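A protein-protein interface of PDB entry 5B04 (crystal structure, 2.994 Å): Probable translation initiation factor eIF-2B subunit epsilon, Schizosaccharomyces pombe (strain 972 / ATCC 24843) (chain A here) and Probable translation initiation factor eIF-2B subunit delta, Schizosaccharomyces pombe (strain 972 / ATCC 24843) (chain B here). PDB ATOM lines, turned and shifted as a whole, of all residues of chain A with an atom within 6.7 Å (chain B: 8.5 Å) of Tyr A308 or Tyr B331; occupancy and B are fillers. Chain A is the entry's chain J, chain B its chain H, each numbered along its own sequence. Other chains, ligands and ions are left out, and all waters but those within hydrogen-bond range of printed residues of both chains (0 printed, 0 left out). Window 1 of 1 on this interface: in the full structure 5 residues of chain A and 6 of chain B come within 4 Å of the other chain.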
ATOM      1  N   LEU A 288      22.115 -33.205  -1.118  1.00  0.00           N
ATOM      2  CA  LEU A 288      20.995 -32.595  -1.830  1.00  0.00           C
ATOM      3  C   LEU A 288      21.438 -32.206  -3.235  1.00  0.00           C
ATOM      4  O   LEU A 288      20.723 -32.439  -4.209  1.00  0.00           O
ATOM      5  CB  LEU A 288      20.455 -31.383  -1.072  1.00  0.00           C
ATOM      6  CG  LEU A 288      19.682 -31.718   0.205  1.00  0.00           C
ATOM      7  CD1 LEU A 288      18.829 -30.537   0.639  1.00  0.00           C
ATOM      8  CD2 LEU A 288      18.828 -32.965   0.011  1.00  0.00           C
ATOM      9  N   ARG A 290      23.698 -33.275  -6.260  1.00  0.00           N
ATOM     10  CA  ARG A 290      23.842 -34.668  -6.676  1.00  0.00           C
ATOM     11  C   ARG A 290      25.276 -35.201  -6.563  1.00  0.00           C
ATOM     12  O   ARG A 290      25.656 -36.110  -7.299  1.00  0.00           O
ATOM     13  CB  ARG A 290      23.350 -34.825  -8.116  1.00  0.00           C
ATOM     14  CG  ARG A 290      22.103 -34.017  -8.434  1.00  0.00           C
ATOM     15  CD  ARG A 290      20.846 -34.703  -7.939  1.00  0.00           C
ATOM     16  NE  ARG A 290      20.569 -35.919  -8.696  1.00  0.00           N
ATOM     17  CZ  ARG A 290      19.405 -36.560  -8.677  1.00  0.00           C
ATOM     18  NH1 ARG A 290      18.405 -36.096  -7.942  1.00  0.00           N
ATOM     19  NH2 ARG A 290      19.240 -37.661  -9.397  1.00  0.00           N
ATOM     20  N   VAL A 296      21.207 -40.601  -3.585  1.00  0.00           N
ATOM     21  CA  VAL A 296      20.515 -39.321  -3.632  1.00  0.00           C
ATOM     22  C   VAL A 296      19.051 -39.561  -3.267  1.00  0.00           C
ATOM     23  O   VAL A 296      18.467 -40.546  -3.717  1.00  0.00           O
ATOM     24  CB  VAL A 296      20.642 -38.680  -5.042  1.00  0.00           C
ATOM     25  CG1 VAL A 296      19.725 -37.481  -5.202  1.00  0.00           C
ATOM     26  CG2 VAL A 296      22.087 -38.292  -5.326  1.00  0.00           C
ATOM     27  N   ASP A 298      16.098 -39.007  -4.167  1.00  0.00           N
ATOM     28  CA  ASP A 298      15.096 -39.466  -5.126  1.00  0.00           C
ATOM     29  C   ASP A 298      15.417 -40.835  -5.723  1.00  0.00           C
ATOM     30  O   ASP A 298      14.697 -41.319  -6.597  1.00  0.00           O
ATOM     31  CB  ASP A 298      14.926 -38.445  -6.253  1.00  0.00           C
ATOM     32  CG  ASP A 298      16.157 -38.333  -7.125  1.00  0.00           C
ATOM     33  OD1 ASP A 298      17.034 -37.508  -6.804  1.00  0.00           O
ATOM     34  OD2 ASP A 298      16.245 -39.067  -8.132  1.00  0.00           O
ATOM     35  N   PHE A 306      10.531 -40.130  -2.985  1.00  0.00           N
ATOM     36  CA  PHE A 306      11.079 -38.820  -3.318  1.00  0.00           C
ATOM     37  C   PHE A 306      11.116 -38.564  -4.818  1.00  0.00           C
ATOM     38  O   PHE A 306      11.245 -39.489  -5.620  1.00  0.00           O
ATOM     39  CB  PHE A 306      12.485 -38.663  -2.741  1.00  0.00           C
ATOM     40  CG  PHE A 306      12.506 -38.280  -1.292  1.00  0.00           C
ATOM     41  CD1 PHE A 306      12.184 -36.992  -0.900  1.00  0.00           C
ATOM     42  CD2 PHE A 306      12.857 -39.203  -0.322  1.00  0.00           C
ATOM     43  CE1 PHE A 306      12.203 -36.633   0.431  1.00  0.00           C
ATOM     44  CE2 PHE A 306      12.879 -38.851   1.012  1.00  0.00           C
ATOM     45  CZ  PHE A 306      12.552 -37.564   1.389  1.00  0.00           C
ATOM     46  N   SER A 307      11.004 -37.292  -5.183  1.00  0.00           N
ATOM     47  CA  SER A 307      11.113 -36.865  -6.570  1.00  0.00           C
ATOM     48  C   SER A 307      11.954 -35.599  -6.646  1.00  0.00           C
ATOM     49  O   SER A 307      11.802 -34.696  -5.823  1.00  0.00           O
ATOM     50  CB  SER A 307       9.731 -36.623  -7.178  1.00  0.00           C
ATOM     51  OG  SER A 307       8.927 -37.787  -7.098  1.00  0.00           O
ATOM     52  N   TYR A 308      12.846 -35.533  -7.629  1.00  0.00           N
ATOM     53  CA  TYR A 308      13.674 -34.348  -7.802  1.00  0.00           C
ATOM     54  C   TYR A 308      12.953 -33.287  -8.622  1.00  0.00           C
ATOM     55  O   TYR A 308      12.301 -33.591  -9.621  1.00  0.00           O
ATOM     56  CB  TYR A 308      15.004 -34.702  -8.471  1.00  0.00           C
ATOM     57  CG  TYR A 308      15.866 -33.493  -8.768  1.00  0.00           C
ATOM     58  CD1 TYR A 308      16.655 -32.919  -7.781  1.00  0.00           C
ATOM     59  CD2 TYR A 308      15.885 -32.923 -10.036  1.00  0.00           C
ATOM     60  CE1 TYR A 308      17.441 -31.813  -8.047  1.00  0.00           C
ATOM     61  CE2 TYR A 308      16.666 -31.816 -10.310  1.00  0.00           C
ATOM     62  CZ  TYR A 308      17.443 -31.266  -9.313  1.00  0.00           C
ATOM     63  OH  TYR A 308      18.223 -30.166  -9.583  1.00  0.00           O
ATOM     64  N   GLN A 309      13.072 -32.039  -8.184  1.00  0.00           N
ATOM     65  CA  GLN A 309      12.557 -30.907  -8.939  1.00  0.00           C
ATOM     66  C   GLN A 309      13.631 -29.835  -9.032  1.00  0.00           C
ATOM     67  O   GLN A 309      14.633 -29.892  -8.318  1.00  0.00           O
ATOM     68  CB  GLN A 309      11.290 -30.352  -8.291  1.00  0.00           C
ATOM     69  CG  GLN A 309      10.055 -31.203  -8.516  1.00  0.00           C
ATOM     70  CD  GLN A 309       9.015 -31.002  -7.436  1.00  0.00           C
ATOM     71  OE1 GLN A 309       9.348 -30.724  -6.285  1.00  0.00           O
ATOM     72  NE2 GLN A 309       7.745 -31.135  -7.802  1.00  0.00           N
ATOM     73  N   ARG A 310      13.421 -28.862  -9.912  1.00  0.00           N
ATOM     74  CA  ARG A 310      14.416 -27.823 -10.155  1.00  0.00           C
ATOM     75  C   ARG A 310      14.741 -27.045  -8.887  1.00  0.00           C
ATOM     76  O   ARG A 310      13.934 -26.990  -7.957  1.00  0.00           O
ATOM     77  CB  ARG A 310      13.937 -26.872 -11.252  1.00  0.00           C
ATOM     78  CG  ARG A 310      13.817 -27.533 -12.612  1.00  0.00           C
ATOM     79  CD  ARG A 310      13.399 -26.546 -13.685  1.00  0.00           C
ATOM     80  NE  ARG A 310      13.213 -27.208 -14.972  1.00  0.00           N
ATOM     81  CZ  ARG A 310      14.173 -27.363 -15.877  1.00  0.00           C
ATOM     82  NH1 ARG A 310      15.391 -26.895 -15.640  1.00  0.00           N
ATOM     83  NH2 ARG A 310      13.915 -27.983 -17.020  1.00  0.00           N
ATOM     84  N   HIS A 311      15.936 -26.462  -8.864  1.00  0.00           N
ATOM     85  CA  HIS A 311      16.457 -25.744  -7.704  1.00  0.00           C
ATOM     86  C   HIS A 311      16.584 -26.674  -6.499  1.00  0.00           C
ATOM     87  O   HIS A 311      16.473 -26.245  -5.351  1.00  0.00           O
ATOM     88  CB  HIS A 311      15.580 -24.533  -7.381  1.00  0.00           C
ATOM     89  CG  HIS A 311      15.147 -23.771  -8.594  1.00  0.00           C
ATOM     90  ND1 HIS A 311      13.896 -23.916  -9.155  1.00  0.00           N
ATOM     91  CD2 HIS A 311      15.805 -22.876  -9.369  1.00  0.00           C
ATOM     92  CE1 HIS A 311      13.798 -23.133 -10.215  1.00  0.00           C
ATOM     93  NE2 HIS A 311      14.943 -22.492 -10.367  1.00  0.00           N
ATOM     94  N   GLN A 312      16.813 -27.953  -6.790  1.00  0.00           N
ATOM     95  CA  GLN A 312      17.165 -28.958  -5.789  1.00  0.00           C
ATOM     96  C   GLN A 312      16.155 -29.116  -4.656  1.00  0.00           C
ATOM     97  O   GLN A 312      16.540 -29.222  -3.492  1.00  0.00           O
ATOM     98  CB  GLN A 312      18.536 -28.633  -5.192  1.00  0.00           C
ATOM     99  CG  GLN A 312      19.662 -28.607  -6.207  1.00  0.00           C
ATOM    100  CD  GLN A 312      20.856 -27.812  -5.722  1.00  0.00           C
ATOM    101  OE1 GLN A 312      21.252 -26.828  -6.345  1.00  0.00           O
ATOM    102  NE2 GLN A 312      21.434 -28.232  -4.603  1.00  0.00           N
ATOM    103  N   ILE A 313      14.868 -29.142  -4.986  1.00  0.00           N
ATOM    104  CA  ILE A 313      13.862 -29.425  -3.969  1.00  0.00           C
ATOM    105  C   ILE A 313      13.372 -30.869  -4.100  1.00  0.00           C
ATOM    106  O   ILE A 313      13.049 -31.338  -5.193  1.00  0.00           O
ATOM    107  CB  ILE A 313      12.671 -28.432  -4.033  1.00  0.00           C
ATOM    108  CG1 ILE A 313      11.919 -28.533  -5.359  1.00  0.00           C
ATOM    109  CG2 ILE A 313      13.156 -27.008  -3.821  1.00  0.00           C
ATOM    110  CD1 ILE A 313      10.638 -27.726  -5.392  1.00  0.00           C
ATOM    111  N   TYR A 314      13.352 -31.575  -2.975  1.00  0.00           N
ATOM    112  CA  TYR A 314      12.984 -32.987  -2.955  1.00  0.00           C
ATOM    113  C   TYR A 314      11.683 -33.204  -2.189  1.00  0.00           C
ATOM    114  O   TYR A 314      11.566 -32.819  -1.026  1.00  0.00           O
ATOM    115  CB  TYR A 314      14.101 -33.826  -2.327  1.00  0.00           C
ATOM    116  CG  TYR A 314      15.416 -33.794  -3.078  1.00  0.00           C
ATOM    117  CD1 TYR A 314      16.340 -32.780  -2.861  1.00  0.00           C
ATOM    118  CD2 TYR A 314      15.739 -34.790  -3.992  1.00  0.00           C
ATOM    119  CE1 TYR A 314      17.545 -32.752  -3.540  1.00  0.00           C
ATOM    120  CE2 TYR A 314      16.941 -34.770  -4.676  1.00  0.00           C
ATOM    121  CZ  TYR A 314      17.840 -33.750  -4.446  1.00  0.00           C
ATOM    122  OH  TYR A 314      19.036 -33.726  -5.125  1.00  0.00           O
ATOM    123  N   LYS A 315      10.709 -33.828  -2.842  1.00  0.00           N
ATOM    124  CA  LYS A 315       9.410 -34.061  -2.220  1.00  0.00           C
ATOM    125  C   LYS A 315       8.971 -35.517  -2.312  1.00  0.00           C
ATOM    126  O   LYS A 315       8.987 -36.116  -3.387  1.00  0.00           O
ATOM    127  CB  LYS A 315       8.347 -33.163  -2.858  1.00  0.00           C
ATOM    128  CG  LYS A 315       7.821 -32.070  -1.941  1.00  0.00           C
ATOM    129  CD  LYS A 315       6.816 -31.180  -2.659  1.00  0.00           C
ATOM    130  CE  LYS A 315       7.484 -30.376  -3.762  1.00  0.00           C
ATOM    131  NZ  LYS A 315       6.544 -29.422  -4.415  1.00  0.00           N
ATOM    132  N   VAL B 297      22.509 -18.009 -15.860  1.00  0.00           N
ATOM    133  CA  VAL B 297      22.823 -19.362 -16.298  1.00  0.00           C
ATOM    134  C   VAL B 297      24.054 -19.345 -17.200  1.00  0.00           C
ATOM    135  O   VAL B 297      24.000 -18.859 -18.330  1.00  0.00           O
ATOM    136  CB  VAL B 297      21.647 -20.011 -17.050  1.00  0.00           C
ATOM    137  CG1 VAL B 297      22.080 -21.327 -17.677  1.00  0.00           C
ATOM    138  CG2 VAL B 297      20.469 -20.220 -16.111  1.00  0.00           C
ATOM    139  N   THR B 322      24.028 -20.450 -12.237  1.00  0.00           N
ATOM    140  CA  THR B 322      23.822 -21.868 -12.501  1.00  0.00           C
ATOM    141  C   THR B 322      24.762 -22.293 -13.626  1.00  0.00           C
ATOM    142  O   THR B 322      24.869 -21.606 -14.642  1.00  0.00           O
ATOM    143  CB  THR B 322      22.363 -22.179 -12.887  1.00  0.00           C
ATOM    144  OG1 THR B 322      21.494 -21.832 -11.801  1.00  0.00           O
ATOM    145  CG2 THR B 322      22.196 -23.657 -13.209  1.00  0.00           C
ATOM    146  N   VAL B 324      25.958 -25.155 -16.390  1.00  0.00           N
ATOM    147  CA  VAL B 324      25.627 -26.355 -17.155  1.00  0.00           C
ATOM    148  C   VAL B 324      26.449 -26.461 -18.436  1.00  0.00           C
ATOM    149  O   VAL B 324      27.043 -25.482 -18.888  1.00  0.00           O
ATOM    150  CB  VAL B 324      24.132 -26.395 -17.538  1.00  0.00           C
ATOM    151  CG1 VAL B 324      23.253 -26.458 -16.297  1.00  0.00           C
ATOM    152  CG2 VAL B 324      23.775 -25.192 -18.399  1.00  0.00           C
ATOM    153  N   MET B 325      26.477 -27.657 -19.016  1.00  0.00           N
ATOM    154  CA  MET B 325      27.102 -27.861 -20.318  1.00  0.00           C
ATOM    155  C   MET B 325      26.089 -27.591 -21.423  1.00  0.00           C
ATOM    156  O   MET B 325      24.884 -27.558 -21.174  1.00  0.00           O
ATOM    157  CB  MET B 325      27.660 -29.280 -20.441  1.00  0.00           C
ATOM    158  CG  MET B 325      28.852 -29.550 -19.544  1.00  0.00           C
ATOM    159  SD  MET B 325      30.265 -28.513 -19.960  1.00  0.00           S
ATOM    160  CE  MET B 325      31.175 -28.568 -18.420  1.00  0.00           C
ATOM    161  N   ILE B 326      26.582 -27.406 -22.644  1.00  0.00           N
ATOM    162  CA  ILE B 326      25.723 -27.046 -23.768  1.00  0.00           C
ATOM    163  C   ILE B 326      24.761 -28.181 -24.126  1.00  0.00           C
ATOM    164  O   ILE B 326      23.734 -27.956 -24.763  1.00  0.00           O
ATOM    165  CB  ILE B 326      26.560 -26.660 -25.011  1.00  0.00           C
ATOM    166  CG1 ILE B 326      25.695 -25.926 -26.041  1.00  0.00           C
ATOM    167  CG2 ILE B 326      27.231 -27.885 -25.617  1.00  0.00           C
ATOM    168  CD1 ILE B 326      26.455 -25.461 -27.263  1.00  0.00           C
ATOM    169  N   SER B 327      25.087 -29.397 -23.700  1.00  0.00           N
ATOM    170  CA  SER B 327      24.226 -30.546 -23.957  1.00  0.00           C
ATOM    171  C   SER B 327      22.969 -30.489 -23.094  1.00  0.00           C
ATOM    172  O   SER B 327      21.944 -31.081 -23.431  1.00  0.00           O
ATOM    173  CB  SER B 327      24.982 -31.851 -23.704  1.00  0.00           C
ATOM    174  OG  SER B 327      25.341 -31.976 -22.340  1.00  0.00           O
ATOM    175  N   ALA B 328      23.057 -29.768 -21.981  1.00  0.00           N
ATOM    176  CA  ALA B 328      21.936 -29.630 -21.057  1.00  0.00           C
ATOM    177  C   ALA B 328      21.092 -28.409 -21.395  1.00  0.00           C
ATOM    178  O   ALA B 328      20.246 -27.991 -20.601  1.00  0.00           O
ATOM    179  CB  ALA B 328      22.440 -29.541 -19.629  1.00  0.00           C
ATOM    180  N   LEU B 329      21.330 -27.845 -22.575  1.00  0.00           N
ATOM    181  CA  LEU B 329      20.684 -26.606 -23.001  1.00  0.00           C
ATOM    182  C   LEU B 329      19.164 -26.689 -22.931  1.00  0.00           C
ATOM    183  O   LEU B 329      18.517 -25.795 -22.392  1.00  0.00           O
ATOM    184  CB  LEU B 329      21.120 -26.248 -24.422  1.00  0.00           C
ATOM    185  CG  LEU B 329      20.852 -24.817 -24.888  1.00  0.00           C
ATOM    186  CD1 LEU B 329      21.480 -23.819 -23.930  1.00  0.00           C
ATOM    187  CD2 LEU B 329      21.381 -24.615 -26.298  1.00  0.00           C
ATOM    188  N   SER B 330      18.607 -27.768 -23.474  1.00  0.00           N
ATOM    189  CA  SER B 330      17.162 -27.980 -23.484  1.00  0.00           C
ATOM    190  C   SER B 330      16.572 -27.933 -22.081  1.00  0.00           C
ATOM    191  O   SER B 330      15.546 -27.292 -21.847  1.00  0.00           O
ATOM    192  CB  SER B 330      16.830 -29.322 -24.136  1.00  0.00           C
ATOM    193  OG  SER B 330      17.527 -30.381 -23.505  1.00  0.00           O
ATOM    194  N   TYR B 331      17.234 -28.614 -21.152  1.00  0.00           N
ATOM    195  CA  TYR B 331      16.790 -28.681 -19.765  1.00  0.00           C
ATOM    196  C   TYR B 331      16.781 -27.306 -19.107  1.00  0.00           C
ATOM    197  O   TYR B 331      15.776 -26.888 -18.533  1.00  0.00           O
ATOM    198  CB  TYR B 331      17.686 -29.642 -18.975  1.00  0.00           C
ATOM    199  CG  TYR B 331      17.360 -29.741 -17.500  1.00  0.00           C
ATOM    200  CD1 TYR B 331      16.363 -30.592 -17.045  1.00  0.00           C
ATOM    201  CD2 TYR B 331      18.064 -28.996 -16.561  1.00  0.00           C
ATOM    202  CE1 TYR B 331      16.065 -30.690 -15.698  1.00  0.00           C
ATOM    203  CE2 TYR B 331      17.774 -29.087 -15.213  1.00  0.00           C
ATOM    204  CZ  TYR B 331      16.774 -29.935 -14.787  1.00  0.00           C
ATOM    205  OH  TYR B 331      16.481 -30.029 -13.445  1.00  0.00           O
ATOM    206  N   ILE B 332      17.903 -26.601 -19.204  1.00  0.00           N
ATOM    207  CA  ILE B 332      18.080 -25.341 -18.492  1.00  0.00           C
ATOM    208  C   ILE B 332      17.394 -24.164 -19.191  1.00  0.00           C
ATOM    209  O   ILE B 332      17.193 -23.110 -18.586  1.00  0.00           O
ATOM    210  CB  ILE B 332      19.583 -25.020 -18.311  1.00  0.00           C
ATOM    211  CG1 ILE B 332      19.791 -24.037 -17.157  1.00  0.00           C
ATOM    212  CG2 ILE B 332      20.187 -24.500 -19.612  1.00  0.00           C
ATOM    213  CD1 ILE B 332      19.183 -24.491 -15.849  1.00  0.00           C
ATOM    214  N   MET B 333      17.022 -24.347 -20.454  1.00  0.00           N
ATOM    215  CA  MET B 333      16.410 -23.270 -21.230  1.00  0.00           C
ATOM    216  C   MET B 333      15.035 -22.892 -20.683  1.00  0.00           C
ATOM    217  O   MET B 333      14.567 -21.770 -20.880  1.00  0.00           O
ATOM    218  CB  MET B 333      16.297 -23.666 -22.704  1.00  0.00           C
ATOM    219  CG  MET B 333      15.862 -22.537 -23.628  1.00  0.00           C
ATOM    220  SD  MET B 333      16.913 -21.076 -23.497  1.00  0.00           S
ATOM    221  CE  MET B 333      18.434 -21.681 -24.223  1.00  0.00           C
ATOM    222  N   GLN B 334      14.398 -23.825 -19.983  1.00  0.00           N
ATOM    223  CA  GLN B 334      13.056 -23.599 -19.453  1.00  0.00           C
ATOM    224  C   GLN B 334      13.048 -22.670 -18.240  1.00  0.00           C
ATOM    225  O   GLN B 334      11.989 -22.363 -17.695  1.00  0.00           O
ATOM    226  CB  GLN B 334      12.399 -24.932 -19.088  1.00  0.00           C
ATOM    227  CG  GLN B 334      12.112 -25.826 -20.283  1.00  0.00           C
ATOM    228  CD  GLN B 334      11.018 -26.837 -20.003  1.00  0.00           C
ATOM    229  OE1 GLN B 334      10.183 -27.119 -20.863  1.00  0.00           O
ATOM    230  NE2 GLN B 334      11.016 -27.390 -18.795  1.00  0.00           N
ATOM    231  N   GLU B 335      14.228 -22.222 -17.823  1.00  0.00           N
ATOM    232  CA  GLU B 335      14.342 -21.295 -16.703  1.00  0.00           C
ATOM    233  C   GLU B 335      14.781 -19.915 -17.178  1.00  0.00           C
ATOM    234  O   GLU B 335      14.662 -18.929 -16.451  1.00  0.00           O
ATOM    235  CB  GLU B 335      15.330 -21.823 -15.662  1.00  0.00           C
ATOM    236  CG  GLU B 335      14.925 -23.136 -15.019  1.00  0.00           C
ATOM    237  CD  GLU B 335      15.984 -23.669 -14.074  1.00  0.00           C
ATOM    238  OE1 GLU B 335      16.539 -22.872 -13.290  1.00  0.00           O
ATOM    239  OE2 GLU B 335      16.262 -24.886 -14.118  1.00  0.00           O
ATOM    240  N   VAL B 336      15.284 -19.855 -18.406  1.00  0.00           N
ATOM    241  CA  VAL B 336      15.865 -18.632 -18.950  1.00  0.00           C
ATOM    242  C   VAL B 336      14.809 -17.626 -19.398  1.00  0.00           C
ATOM    243  O   VAL B 336      13.836 -17.985 -20.063  1.00  0.00           O
ATOM    244  CB  VAL B 336      16.788 -18.946 -20.142  1.00  0.00           C
ATOM    245  CG1 VAL B 336      17.500 -17.689 -20.612  1.00  0.00           C
ATOM    246  CG2 VAL B 336      17.793 -20.020 -19.759  1.00  0.00           C
ATOM    247  N   LEU B 364      17.723 -22.858 -29.746  1.00  0.00           N
ATOM    248  CA  LEU B 364      16.905 -23.381 -28.658  1.00  0.00           C
ATOM    249  C   LEU B 364      16.249 -22.248 -27.877  1.00  0.00           C
ATOM    250  O   LEU B 364      15.174 -22.421 -27.304  1.00  0.00           O
ATOM    251  CB  LEU B 364      17.739 -24.256 -27.721  1.00  0.00           C
ATOM    252  CG  LEU B 364      17.761 -25.753 -28.043  1.00  0.00           C
ATOM    253  CD1 LEU B 364      18.585 -26.033 -29.290  1.00  0.00           C
ATOM    254  CD2 LEU B 364      18.277 -26.554 -26.858  1.00  0.00           C
ATOM    255  N   SER B 368      11.957 -21.545 -27.225  1.00  0.00           N
ATOM    256  CA  SER B 368      11.400 -21.300 -25.900  1.00  0.00           C
ATOM    257  C   SER B 368      11.006 -19.835 -25.730  1.00  0.00           C
ATOM    258  O   SER B 368      10.815 -19.364 -24.608  1.00  0.00           O
ATOM    259  CB  SER B 368      12.398 -21.707 -24.815  1.00  0.00           C
ATOM    260  OG  SER B 368      12.726 -23.082 -24.919  1.00  0.00           O
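The side-chain carboxylate (OE1) of Glu B335 lies within hydrogen-bond range of a ring nitrogen (NE2) of His A311 (3.4 Å).
O of Tyr B331 lies within hydrogen-bond range of NH2 of Arg A310.
NE2 of Gln B334 lies close to NH2 of Arg A310 (3.5 Å).
The guanidinium group (NH1) of Arg A310 is in salt-bridge range of the side-chain carboxylate (OE2) of Glu B335, at 2.7 Å.
Hydrophobic or aromatic side chains of chain B within 4 Å of the printed part of chain A: Tyr B331.
Among the printed residues, Asp or Glu carboxylates within 4 Å of a Lys or Arg side-chain nitrogen of the other chain: Arg A310 with Glu B335 (2.7 Å).
Tyr B331 touches two residues of chain A.
Of the printed residues of chain A, Gln B334 touches Arg A310 (3.5 Å).
Printed residues of chain B within 4 Å of Arg A310: Tyr B331 (2.6 Å), Gln B334 (3.5 Å) and Glu B335 (2.7 Å).
Printed residues of chain B within 4 Å of His A311: Glu B335 (3.4 Å).
Printed residues of chain A within 4 Å of Glu B335: Arg A310 and His A311.
The nearest residue of chain B that does not touch Tyr A308 is Glu B335 (7.2 Å).
The nearest residue of chain A that does not touch Tyr B331 is Gln A309 (5.3 Å).
Among the printed residues, pairs that only touch across the chains: Tyr A308 with Tyr B331 (3.6 Å).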
